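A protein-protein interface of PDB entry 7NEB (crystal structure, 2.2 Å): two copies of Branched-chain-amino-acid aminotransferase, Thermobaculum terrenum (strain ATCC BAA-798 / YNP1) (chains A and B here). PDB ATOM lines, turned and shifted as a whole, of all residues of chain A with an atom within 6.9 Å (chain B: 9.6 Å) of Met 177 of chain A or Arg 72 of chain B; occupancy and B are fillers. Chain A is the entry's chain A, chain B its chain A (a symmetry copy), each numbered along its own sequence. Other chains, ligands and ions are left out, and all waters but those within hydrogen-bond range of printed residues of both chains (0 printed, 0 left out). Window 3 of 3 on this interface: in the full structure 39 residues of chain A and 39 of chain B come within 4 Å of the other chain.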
ATOM      1  N   TRP A 147      20.993  36.305  -3.366  1.00  0.00           N
ATOM      2  CA  TRP A 147      20.753  35.303  -4.435  1.00  0.00           C
ATOM      3  C   TRP A 147      19.985  35.922  -5.633  1.00  0.00           C
ATOM      4  O   TRP A 147      18.953  36.578  -5.434  1.00  0.00           O
ATOM      5  CB  TRP A 147      20.021  34.094  -3.864  1.00  0.00           C
ATOM      6  CG  TRP A 147      20.738  33.450  -2.722  1.00  0.00           C
ATOM      7  CD1 TRP A 147      20.483  33.659  -1.399  1.00  0.00           C
ATOM      8  CD2 TRP A 147      21.819  32.501  -2.792  1.00  0.00           C
ATOM      9  NE1 TRP A 147      21.386  32.972  -0.633  1.00  0.00           N
ATOM     10  CE2 TRP A 147      22.203  32.232  -1.448  1.00  0.00           C
ATOM     11  CE3 TRP A 147      22.537  31.893  -3.843  1.00  0.00           C
ATOM     12  CZ2 TRP A 147      23.207  31.313  -1.128  1.00  0.00           C
ATOM     13  CZ3 TRP A 147      23.581  31.044  -3.526  1.00  0.00           C
ATOM     14  CH2 TRP A 147      23.906  30.756  -2.184  1.00  0.00           C
ATOM     15  N   ARG A 166      13.150  26.215  -6.039  1.00  0.00           N
ATOM     16  CA  ARG A 166      14.421  26.003  -5.294  1.00  0.00           C
ATOM     17  C   ARG A 166      15.123  27.375  -5.183  1.00  0.00           C
ATOM     18  O   ARG A 166      15.579  27.731  -4.088  1.00  0.00           O
ATOM     19  CB  ARG A 166      15.271  24.947  -6.007  1.00  0.00           C
ATOM     20  CG  ARG A 166      16.659  24.704  -5.410  1.00  0.00           C
ATOM     21  CD  ARG A 166      16.640  23.805  -4.189  1.00  0.00           C
ATOM     22  NE  ARG A 166      16.052  24.396  -2.971  1.00  0.00           N
ATOM     23  CZ  ARG A 166      16.698  25.218  -2.102  1.00  0.00           C
ATOM     24  NH1 ARG A 166      17.964  25.581  -2.301  1.00  0.00           N
ATOM     25  NH2 ARG A 166      16.067  25.698  -1.033  1.00  0.00           N
ATOM     26  N   GLN A 169      13.553  29.625  -2.596  1.00  0.00           N
ATOM     27  CA  GLN A 169      13.794  29.333  -1.128  1.00  0.00           C
ATOM     28  C   GLN A 169      15.256  29.618  -0.687  1.00  0.00           C
ATOM     29  O   GLN A 169      15.503  29.658   0.537  1.00  0.00           O
ATOM     30  CB  GLN A 169      13.233  27.960  -0.762  1.00  0.00           C
ATOM     31  CG  GLN A 169      11.752  27.853  -1.091  1.00  0.00           C
ATOM     32  CD  GLN A 169      11.147  26.485  -0.893  1.00  0.00           C
ATOM     33  OE1 GLN A 169      11.840  25.495  -0.663  1.00  0.00           O
ATOM     34  NE2 GLN A 169       9.829  26.425  -1.025  1.00  0.00           N
ATOM     35  N   LEU A 170      16.210  29.826  -1.617  1.00  0.00           N
ATOM     36  CA  LEU A 170      17.504  30.522  -1.312  1.00  0.00           C
ATOM     37  C   LEU A 170      17.174  31.908  -0.691  1.00  0.00           C
ATOM     38  O   LEU A 170      17.637  32.228   0.416  1.00  0.00           O
ATOM     39  CB  LEU A 170      18.356  30.699  -2.589  1.00  0.00           C
ATOM     40  CG  LEU A 170      18.902  29.430  -3.258  1.00  0.00           C
ATOM     41  CD1 LEU A 170      19.492  29.754  -4.657  1.00  0.00           C
ATOM     42  CD2 LEU A 170      19.934  28.742  -2.338  1.00  0.00           C
ATOM     43  N   SER A 172      14.024  33.133   0.259  1.00  0.00           N
ATOM     44  CA  SER A 172      12.991  33.181   1.324  1.00  0.00           C
ATOM     45  C   SER A 172      13.578  32.780   2.691  1.00  0.00           C
ATOM     46  O   SER A 172      13.186  33.407   3.681  1.00  0.00           O
ATOM     47  CB  SER A 172      11.768  32.386   0.942  1.00  0.00           C
ATOM     48  OG  SER A 172      12.163  31.219   0.250  1.00  0.00           O
ATOM     49  N   SER A 173      14.480  31.804   2.763  1.00  0.00           N
ATOM     50  CA  SER A 173      15.113  31.351   4.044  1.00  0.00           C
ATOM     51  C   SER A 173      16.156  32.402   4.469  1.00  0.00           C
ATOM     52  O   SER A 173      16.155  32.701   5.640  1.00  0.00           O
ATOM     53  CB  SER A 173      15.705  29.915   4.015  1.00  0.00           C
ATOM     54  OG  SER A 173      15.696  29.274   5.325  1.00  0.00           O
ATOM     55  N   GLU A 174      16.941  32.982   3.540  1.00  0.00           N
ATOM     56  CA  GLU A 174      17.835  34.150   3.818  1.00  0.00           C
ATOM     57  C   GLU A 174      17.013  35.254   4.528  1.00  0.00           C
ATOM     58  O   GLU A 174      17.440  35.763   5.574  1.00  0.00           O
ATOM     59  CB  GLU A 174      18.482  34.692   2.523  1.00  0.00           C
ATOM     60  CG  GLU A 174      19.219  36.046   2.689  1.00  0.00           C
ATOM     61  CD  GLU A 174      19.941  36.522   1.447  1.00  0.00           C
ATOM     62  OE1 GLU A 174      19.288  36.643   0.407  1.00  0.00           O
ATOM     63  OE2 GLU A 174      21.155  36.715   1.498  1.00  0.00           O
ATOM     64  N   ALA A 175      15.855  35.596   3.966  1.00  0.00           N
ATOM     65  CA  ALA A 175      15.012  36.734   4.375  1.00  0.00           C
ATOM     66  C   ALA A 175      14.580  36.522   5.825  1.00  0.00           C
ATOM     67  O   ALA A 175      14.794  37.454   6.656  1.00  0.00           O
ATOM     68  CB  ALA A 175      13.866  36.911   3.425  1.00  0.00           C
ATOM     69  N   ALA A 176      14.117  35.321   6.144  1.00  0.00           N
ATOM     70  CA  ALA A 176      13.649  34.958   7.503  1.00  0.00           C
ATOM     71  C   ALA A 176      14.824  34.984   8.497  1.00  0.00           C
ATOM     72  O   ALA A 176      14.644  35.518   9.637  1.00  0.00           O
ATOM     73  CB  ALA A 176      12.994  33.586   7.469  1.00  0.00           C
ATOM     74  N   MET A 177      15.987  34.388   8.155  1.00  0.00           N
ATOM     75  CA  MET A 177      17.079  34.297   9.166  1.00  0.00           C
ATOM     76  C   MET A 177      17.679  35.716   9.406  1.00  0.00           C
ATOM     77  O   MET A 177      18.210  35.945  10.494  1.00  0.00           O
ATOM     78  CB  MET A 177      18.143  33.242   8.804  1.00  0.00           C
ATOM     79  CG  MET A 177      19.331  33.778   8.017  1.00  0.00           C
ATOM     80  SD  MET A 177      20.461  32.516   7.393  1.00  0.00           S
ATOM     81  CE  MET A 177      19.429  31.819   6.098  1.00  0.00           C
ATOM     82  N   ASN A 178      17.591  36.634   8.433  1.00  0.00           N
ATOM     83  CA  ASN A 178      18.055  38.035   8.561  1.00  0.00           C
ATOM     84  C   ASN A 178      16.904  38.952   8.995  1.00  0.00           C
ATOM     85  O   ASN A 178      17.038  40.153   8.780  1.00  0.00           O
ATOM     86  CB  ASN A 178      18.685  38.524   7.256  1.00  0.00           C
ATOM     87  CG  ASN A 178      19.872  37.728   6.771  1.00  0.00           C
ATOM     88  OD1 ASN A 178      20.273  37.828   5.603  1.00  0.00           O
ATOM     89  ND2 ASN A 178      20.470  36.940   7.630  1.00  0.00           N
ATOM     90  N   GLY A 179      15.815  38.449   9.572  1.00  0.00           N
ATOM     91  CA  GLY A 179      14.834  39.300  10.280  1.00  0.00           C
ATOM     92  C   GLY A 179      13.849  39.994   9.349  1.00  0.00           C
ATOM     93  O   GLY A 179      13.198  40.935   9.788  1.00  0.00           O
ATOM     94  N   TYR A 180      13.719  39.598   8.088  1.00  0.00           N
ATOM     95  CA  TYR A 180      12.688  40.152   7.175  1.00  0.00           C
ATOM     96  C   TYR A 180      11.532  39.161   7.006  1.00  0.00           C
ATOM     97  O   TYR A 180      11.733  37.966   7.226  1.00  0.00           O
ATOM     98  CB  TYR A 180      13.334  40.461   5.832  1.00  0.00           C
ATOM     99  CG  TYR A 180      14.406  41.507   5.887  1.00  0.00           C
ATOM    100  CD1 TYR A 180      14.118  42.862   5.769  1.00  0.00           C
ATOM    101  CD2 TYR A 180      15.716  41.133   6.062  1.00  0.00           C
ATOM    102  CE1 TYR A 180      15.117  43.827   5.852  1.00  0.00           C
ATOM    103  CE2 TYR A 180      16.734  42.072   6.089  1.00  0.00           C
ATOM    104  CZ  TYR A 180      16.433  43.422   5.992  1.00  0.00           C
ATOM    105  OH  TYR A 180      17.461  44.320   5.981  1.00  0.00           O
ATOM    106  N   THR B  35      13.039  21.186  -2.145  1.00  0.00           N
ATOM    107  CA  THR B  35      14.179  21.246  -1.159  1.00  0.00           C
ATOM    108  C   THR B  35      15.093  20.019  -1.289  1.00  0.00           C
ATOM    109  O   THR B  35      16.157  19.998  -0.661  1.00  0.00           O
ATOM    110  CB  THR B  35      13.662  21.070   0.284  1.00  0.00           C
ATOM    111  OG1 THR B  35      13.265  19.684   0.633  1.00  0.00           O
ATOM    112  CG2 THR B  35      12.562  22.086   0.520  1.00  0.00           C
ATOM    113  N   VAL B  37      17.316  16.714  -1.708  1.00  0.00           N
ATOM    114  CA  VAL B  37      18.676  16.395  -2.131  1.00  0.00           C
ATOM    115  C   VAL B  37      18.814  14.897  -2.023  1.00  0.00           C
ATOM    116  O   VAL B  37      18.090  14.264  -1.294  1.00  0.00           O
ATOM    117  CB  VAL B  37      19.722  17.177  -1.323  1.00  0.00           C
ATOM    118  CG1 VAL B  37      19.557  18.669  -1.540  1.00  0.00           C
ATOM    119  CG2 VAL B  37      19.708  16.874   0.119  1.00  0.00           C
ATOM    120  N   LEU B  64      25.959  14.119   1.171  1.00  0.00           N
ATOM    121  CA  LEU B  64      24.517  14.324   1.456  1.00  0.00           C
ATOM    122  C   LEU B  64      24.373  15.268   2.654  1.00  0.00           C
ATOM    123  O   LEU B  64      23.510  16.194   2.619  1.00  0.00           O
ATOM    124  CB  LEU B  64      23.882  12.947   1.704  1.00  0.00           C
ATOM    125  CG  LEU B  64      22.401  12.957   2.065  1.00  0.00           C
ATOM    126  CD1 LEU B  64      21.623  13.541   0.896  1.00  0.00           C
ATOM    127  CD2 LEU B  64      21.898  11.547   2.465  1.00  0.00           C
ATOM    128  N   GLU B  65      25.123  15.026   3.736  1.00  0.00           N
ATOM    129  CA  GLU B  65      24.994  15.876   4.946  1.00  0.00           C
ATOM    130  C   GLU B  65      25.320  17.335   4.587  1.00  0.00           C
ATOM    131  O   GLU B  65      24.586  18.239   5.038  1.00  0.00           O
ATOM    132  CB  GLU B  65      25.904  15.392   6.059  1.00  0.00           C
ATOM    133  CG  GLU B  65      25.991  16.387   7.247  1.00  0.00           C
ATOM    134  CD  GLU B  65      27.357  16.279   7.902  1.00  0.00           C
ATOM    135  OE1 GLU B  65      28.351  16.659   7.232  1.00  0.00           O
ATOM    136  OE2 GLU B  65      27.434  15.687   9.001  1.00  0.00           O
ATOM    137  N   GLN B  66      26.282  17.545   3.703  1.00  0.00           N
ATOM    138  CA  GLN B  66      26.650  18.905   3.248  1.00  0.00           C
ATOM    139  C   GLN B  66      25.554  19.474   2.395  1.00  0.00           C
ATOM    140  O   GLN B  66      25.186  20.595   2.631  1.00  0.00           O
ATOM    141  CB  GLN B  66      27.965  18.843   2.465  1.00  0.00           C
ATOM    142  CG  GLN B  66      29.118  18.501   3.421  1.00  0.00           C
ATOM    143  CD  GLN B  66      30.387  18.202   2.673  1.00  0.00           C
ATOM    144  OE1 GLN B  66      30.483  18.358   1.467  1.00  0.00           O
ATOM    145  NE2 GLN B  66      31.349  17.715   3.423  1.00  0.00           N
ATOM    146  N   SER B  67      25.050  18.714   1.434  1.00  0.00           N
ATOM    147  CA  SER B  67      23.931  19.202   0.599  1.00  0.00           C
ATOM    148  C   SER B  67      22.807  19.596   1.548  1.00  0.00           C
ATOM    149  O   SER B  67      22.166  20.663   1.332  1.00  0.00           O
ATOM    150  CB  SER B  67      23.487  18.219  -0.394  1.00  0.00           C
ATOM    151  OG  SER B  67      24.456  17.976  -1.407  1.00  0.00           O
ATOM    152  N   MET B  68      22.627  18.833   2.629  1.00  0.00           N
ATOM    153  CA  MET B  68      21.498  19.128   3.542  1.00  0.00           C
ATOM    154  C   MET B  68      21.789  20.399   4.307  1.00  0.00           C
ATOM    155  O   MET B  68      20.812  21.153   4.666  1.00  0.00           O
ATOM    156  CB  MET B  68      21.225  17.978   4.518  1.00  0.00           C
ATOM    157  CG  MET B  68      20.565  16.795   3.812  1.00  0.00           C
ATOM    158  SD  MET B  68      20.521  15.236   4.722  1.00  0.00           S
ATOM    159  CE  MET B  68      19.298  15.681   5.936  1.00  0.00           C
ATOM    160  N   GLN B  69      23.044  20.570   4.692  1.00  0.00           N
ATOM    161  CA  GLN B  69      23.420  21.757   5.472  1.00  0.00           C
ATOM    162  C   GLN B  69      23.251  23.013   4.598  1.00  0.00           C
ATOM    163  O   GLN B  69      22.701  24.029   5.091  1.00  0.00           O
ATOM    164  CB  GLN B  69      24.818  21.644   6.051  1.00  0.00           C
ATOM    165  CG  GLN B  69      25.106  22.863   6.929  1.00  0.00           C
ATOM    166  CD  GLN B  69      26.585  22.955   7.197  1.00  0.00           C
ATOM    167  OE1 GLN B  69      27.272  21.920   7.219  1.00  0.00           O
ATOM    168  NE2 GLN B  69      27.060  24.189   7.391  1.00  0.00           N
ATOM    169  N   LEU B  70      23.587  22.937   3.329  1.00  0.00           N
ATOM    170  CA  LEU B  70      23.464  24.102   2.404  1.00  0.00           C
ATOM    171  C   LEU B  70      22.013  24.439   2.069  1.00  0.00           C
ATOM    172  O   LEU B  70      21.687  25.634   1.893  1.00  0.00           O
ATOM    173  CB  LEU B  70      24.268  23.763   1.149  1.00  0.00           C
ATOM    174  CG  LEU B  70      25.768  23.595   1.370  1.00  0.00           C
ATOM    175  CD1 LEU B  70      26.415  23.104   0.099  1.00  0.00           C
ATOM    176  CD2 LEU B  70      26.376  24.914   1.799  1.00  0.00           C
ATOM    177  N   ILE B  71      21.148  23.433   1.993  1.00  0.00           N
ATOM    178  CA  ILE B  71      19.682  23.627   1.864  1.00  0.00           C
ATOM    179  C   ILE B  71      19.191  24.208   3.203  1.00  0.00           C
ATOM    180  O   ILE B  71      18.095  24.669   3.222  1.00  0.00           O
ATOM    181  CB  ILE B  71      18.998  22.284   1.483  1.00  0.00           C
ATOM    182  CG1 ILE B  71      19.352  21.863   0.067  1.00  0.00           C
ATOM    183  CG2 ILE B  71      17.462  22.320   1.618  1.00  0.00           C
ATOM    184  CD1 ILE B  71      18.539  22.572  -1.034  1.00  0.00           C
ATOM    185  N   ARG B  72      19.909  24.020   4.321  1.00  0.00           N
ATOM    186  CA  ARG B  72      19.499  24.416   5.682  1.00  0.00           C
ATOM    187  C   ARG B  72      18.359  23.567   6.200  1.00  0.00           C
ATOM    188  O   ARG B  72      17.481  24.096   6.942  1.00  0.00           O
ATOM    189  CB  ARG B  72      19.173  25.903   5.781  1.00  0.00           C
ATOM    190  CG  ARG B  72      20.409  26.759   5.547  1.00  0.00           C
ATOM    191  CD  ARG B  72      20.034  28.204   5.391  1.00  0.00           C
ATOM    192  NE  ARG B  72      21.024  29.046   4.735  1.00  0.00           N
ATOM    193  CZ  ARG B  72      22.067  29.618   5.344  1.00  0.00           C
ATOM    194  NH1 ARG B  72      22.335  29.408   6.620  1.00  0.00           N
ATOM    195  NH2 ARG B  72      22.802  30.464   4.658  1.00  0.00           N
ATOM    196  N   MET B  73      18.455  22.267   5.968  1.00  0.00           N
ATOM    197  CA  MET B  73      17.606  21.275   6.654  1.00  0.00           C
ATOM    198  C   MET B  73      18.081  21.134   8.102  1.00  0.00           C
ATOM    199  O   MET B  73      19.258  20.919   8.362  1.00  0.00           O
ATOM    200  CB  MET B  73      17.677  19.932   5.960  1.00  0.00           C
ATOM    201  CG  MET B  73      17.040  20.039   4.619  1.00  0.00           C
ATOM    202  SD  MET B  73      17.095  18.425   3.930  1.00  0.00           S
ATOM    203  CE  MET B  73      16.645  18.668   2.215  1.00  0.00           C
ATOM    204  N   PRO B  74      17.191  21.239   9.102  1.00  0.00           N
ATOM    205  CA  PRO B  74      17.590  20.993  10.492  1.00  0.00           C
ATOM    206  C   PRO B  74      18.178  19.602  10.672  1.00  0.00           C
ATOM    207  O   PRO B  74      17.836  18.693   9.902  1.00  0.00           O
ATOM    208  CB  PRO B  74      16.306  21.111  11.308  1.00  0.00           C
ATOM    209  CG  PRO B  74      15.407  21.912  10.413  1.00  0.00           C
ATOM    210  CD  PRO B  74      15.776  21.598   8.971  1.00  0.00           C
ATOM    211  N   LYS B  75      19.036  19.469  11.665  1.00  0.00           N
ATOM    212  CA  LYS B  75      19.839  18.252  11.839  1.00  0.00           C
ATOM    213  C   LYS B  75      18.882  17.220  12.423  1.00  0.00           C
ATOM    214  O   LYS B  75      18.119  17.560  13.279  1.00  0.00           O
ATOM    215  CB  LYS B  75      21.154  18.443  12.629  1.00  0.00           C
ATOM    216  CG  LYS B  75      21.939  17.121  12.771  1.00  0.00           C
ATOM    217  CD  LYS B  75      23.430  17.047  12.408  1.00  0.00           C
ATOM    218  CE  LYS B  75      23.719  17.286  10.941  1.00  0.00           C
ATOM    219  NZ  LYS B  75      23.727  16.035  10.142  1.00  0.00           N
ATOM    220  N   GLU B  76      18.931  15.998  11.887  1.00  0.00           N
ATOM    221  CA  GLU B  76      18.013  14.876  12.196  1.00  0.00           C
ATOM    222  C   GLU B  76      18.764  13.567  12.014  1.00  0.00           C
ATOM    223  O   GLU B  76      18.467  12.618  12.744  1.00  0.00           O
ATOM    224  CB  GLU B  76      16.786  14.917  11.258  1.00  0.00           C
ATOM    225  CG  GLU B  76      15.782  13.801  11.544  1.00  0.00           C
ATOM    226  CD  GLU B  76      15.206  13.848  12.948  1.00  0.00           C
ATOM    227  OE1 GLU B  76      14.986  14.979  13.398  1.00  0.00           O
ATOM    228  OE2 GLU B  76      14.960  12.790  13.537  1.00  0.00           O
ATOM    229  N   TYR B 106      14.559  15.462   2.574  1.00  0.00           N
ATOM    230  CA  TYR B 106      13.579  16.497   2.219  1.00  0.00           C
ATOM    231  C   TYR B 106      13.116  17.111   3.527  1.00  0.00           C
ATOM    232  O   TYR B 106      13.071  16.446   4.582  1.00  0.00           O
ATOM    233  CB  TYR B 106      12.464  15.881   1.348  1.00  0.00           C
ATOM    234  CG  TYR B 106      11.663  14.767   2.011  1.00  0.00           C
ATOM    235  CD1 TYR B 106      10.516  15.027   2.757  1.00  0.00           C
ATOM    236  CD2 TYR B 106      12.044  13.455   1.907  1.00  0.00           C
ATOM    237  CE1 TYR B 106       9.798  14.012   3.395  1.00  0.00           C
ATOM    238  CE2 TYR B 106      11.349  12.439   2.563  1.00  0.00           C
ATOM    239  CZ  TYR B 106      10.232  12.699   3.324  1.00  0.00           C
ATOM    240  OH  TYR B 106       9.573  11.700   4.018  1.00  0.00           O
ATOM    241  N   ALA B 107      12.707  18.370   3.434  1.00  0.00           N
ATOM    242  CA  ALA B 107      12.217  19.151   4.572  1.00  0.00           C
ATOM    243  C   ALA B 107      10.722  19.321   4.388  1.00  0.00           C
ATOM    244  O   ALA B 107      10.264  19.710   3.282  1.00  0.00           O
ATOM    245  CB  ALA B 107      12.986  20.438   4.625  1.00  0.00           C
ATOM    246  N   VAL B 108       9.959  19.038   5.425  1.00  0.00           N
ATOM    247  CA  VAL B 108       8.483  19.167   5.378  1.00  0.00           C
ATOM    248  C   VAL B 108       8.083  20.336   6.274  1.00  0.00           C
ATOM    249  O   VAL B 108       8.668  20.472   7.441  1.00  0.00           O
ATOM    250  CB  VAL B 108       7.809  17.849   5.793  1.00  0.00           C
ATOM    251  CG1 VAL B 108       6.295  17.894   5.545  1.00  0.00           C
ATOM    252  CG2 VAL B 108       8.433  16.692   5.039  1.00  0.00           C
ATOM    253  N   GLY B 117       8.362  28.199   8.945  1.00  0.00           N
ATOM    254  CA  GLY B 117       8.796  28.263  10.355  1.00  0.00           C
ATOM    255  C   GLY B 117       9.631  27.054  10.756  1.00  0.00           C
ATOM    256  O   GLY B 117      10.828  27.016  10.396  1.00  0.00           O
ATOM    257  N   ASP B 118       9.026  26.102  11.478  1.00  0.00           N
ATOM    258  CA  ASP B 118       9.699  24.876  11.997  1.00  0.00           C
ATOM    259  C   ASP B 118       9.519  23.736  10.971  1.00  0.00           C
ATOM    260  O   ASP B 118       8.664  22.832  11.191  1.00  0.00           O
ATOM    261  CB  ASP B 118       9.245  24.559  13.431  1.00  0.00           C
ATOM    262  CG  ASP B 118       9.855  25.491  14.472  1.00  0.00           C
ATOM    263  OD1 ASP B 118       9.540  26.701  14.428  1.00  0.00           O
ATOM    264  OD2 ASP B 118      10.662  25.007  15.307  1.00  0.00           O
ATOM    265  N   ARG B 119      10.323  23.774   9.896  1.00  0.00           N
ATOM    266  CA  ARG B 119      10.479  22.654   8.932  1.00  0.00           C
ATOM    267  C   ARG B 119      11.091  21.436   9.667  1.00  0.00           C
ATOM    268  O   ARG B 119      11.895  21.627  10.595  1.00  0.00           O
ATOM    269  CB  ARG B 119      11.191  23.179   7.676  1.00  0.00           C
ATOM    270  CG  ARG B 119      10.319  24.141   6.867  1.00  0.00           C
ATOM    271  CD  ARG B 119      10.904  24.779   5.605  1.00  0.00           C
ATOM    272  NE  ARG B 119      10.497  24.130   4.346  1.00  0.00           N
ATOM    273  CZ  ARG B 119       9.329  24.263   3.684  1.00  0.00           C
ATOM    274  NH1 ARG B 119       8.353  25.036   4.143  1.00  0.00           N
ATOM    275  NH2 ARG B 119       9.141  23.593   2.549  1.00  0.00           N
ATOM    276  N   THR B 120      10.636  20.221   9.338  1.00  0.00           N
ATOM    277  CA  THR B 120      11.182  18.924   9.824  1.00  0.00           C
ATOM    278  C   THR B 120      11.978  18.286   8.658  1.00  0.00           C
ATOM    279  O   THR B 120      11.582  18.403   7.527  1.00  0.00           O
ATOM    280  CB  THR B 120      10.031  18.167  10.518  1.00  0.00           C
ATOM    281  OG1 THR B 120      10.124  18.626  11.870  1.00  0.00           O
ATOM    282  CG2 THR B 120      10.074  16.652  10.538  1.00  0.00           C
ATOM    283  N   THR B 121      13.113  17.673   8.958  1.00  0.00           N
ATOM    284  CA  THR B 121      13.980  16.959   8.020  1.00  0.00           C
ATOM    285  C   THR B 121      13.543  15.519   8.047  1.00  0.00           C
ATOM    286  O   THR B 121      13.554  14.944   9.122  1.00  0.00           O
ATOM    287  CB  THR B 121      15.463  17.033   8.389  1.00  0.00           C
ATOM    288  OG1 THR B 121      15.756  18.421   8.388  1.00  0.00           O
ATOM    289  CG2 THR B 121      16.420  16.307   7.459  1.00  0.00           C
ATOM    290  N   ILE B 159      25.193  21.639  -4.665  1.00  0.00           N
ATOM    291  CA  ILE B 159      24.026  20.936  -4.035  1.00  0.00           C
ATOM    292  C   ILE B 159      23.467  19.979  -5.085  1.00  0.00           C
ATOM    293  O   ILE B 159      23.150  20.426  -6.180  1.00  0.00           O
ATOM    294  CB  ILE B 159      22.930  21.893  -3.511  1.00  0.00           C
ATOM    295  CG1 ILE B 159      23.445  23.042  -2.637  1.00  0.00           C
ATOM    296  CG2 ILE B 159      21.890  21.114  -2.752  1.00  0.00           C
ATOM    297  CD1 ILE B 159      22.555  24.307  -2.657  1.00  0.00           C
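Among the printed residues, merely in contact across the chains: Arg 166 of chain A with Ile 71 of chain B and Gln 169 of chain A with Thr 35 of chain B.
NH1 of Arg 72 of chain B lies within hydrogen-bond range of SD of Met 177 of chain A.
Printed residues of chain B within 4 Å of Arg 166 of chain A: Ile 71 (3.3 Å). Of the printed residues of chain B, Gln 169 of chain A touches Thr 35 (3.7 Å). Met 177 of chain A touches just one residue of chain B: Arg 72 (3.5 Å). No residue of chain B comes within 4 Å of Asn 178 of chain A. Of the printed residues of chain A, Thr 35 of chain B touches Gln 169. Printed residues of chain A within 4 Å of Ile 71 of chain B: Arg 166. Of chain A, only Met 177 (3.5 Å) comes within 4 Å of Arg 72 of chain B. The nearest printed residue of chain B that does not touch Met 177 of chain A is Leu 70 of chain B (7.8 Å). The nearest printed residue of chain A that does not touch Arg 72 of chain B is Ser 173 of chain A (4.5 Å).
Of the 24 printed residues of chain B, 3 touch a printed residue of chain A. Hydrophobic or aromatic side chains of chain A within 4 Å of the printed part of chain B: Met 177. Among the printed residues, 3 pairs touch across the chains. Among the printed residues, no Asp or Glu carboxylate lies within 4 Å of a Lys or Arg side-chain nitrogen of the other chain.
No position is printed for both chains. Of the 3 pairs that touch across the chains among the printed residues, none has its exchanged pair printed and touching as well.
OG1 of Thr 35 of chain B is in hydrogen-bond range of N of Ala 107 of chain B (3.1 Å).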
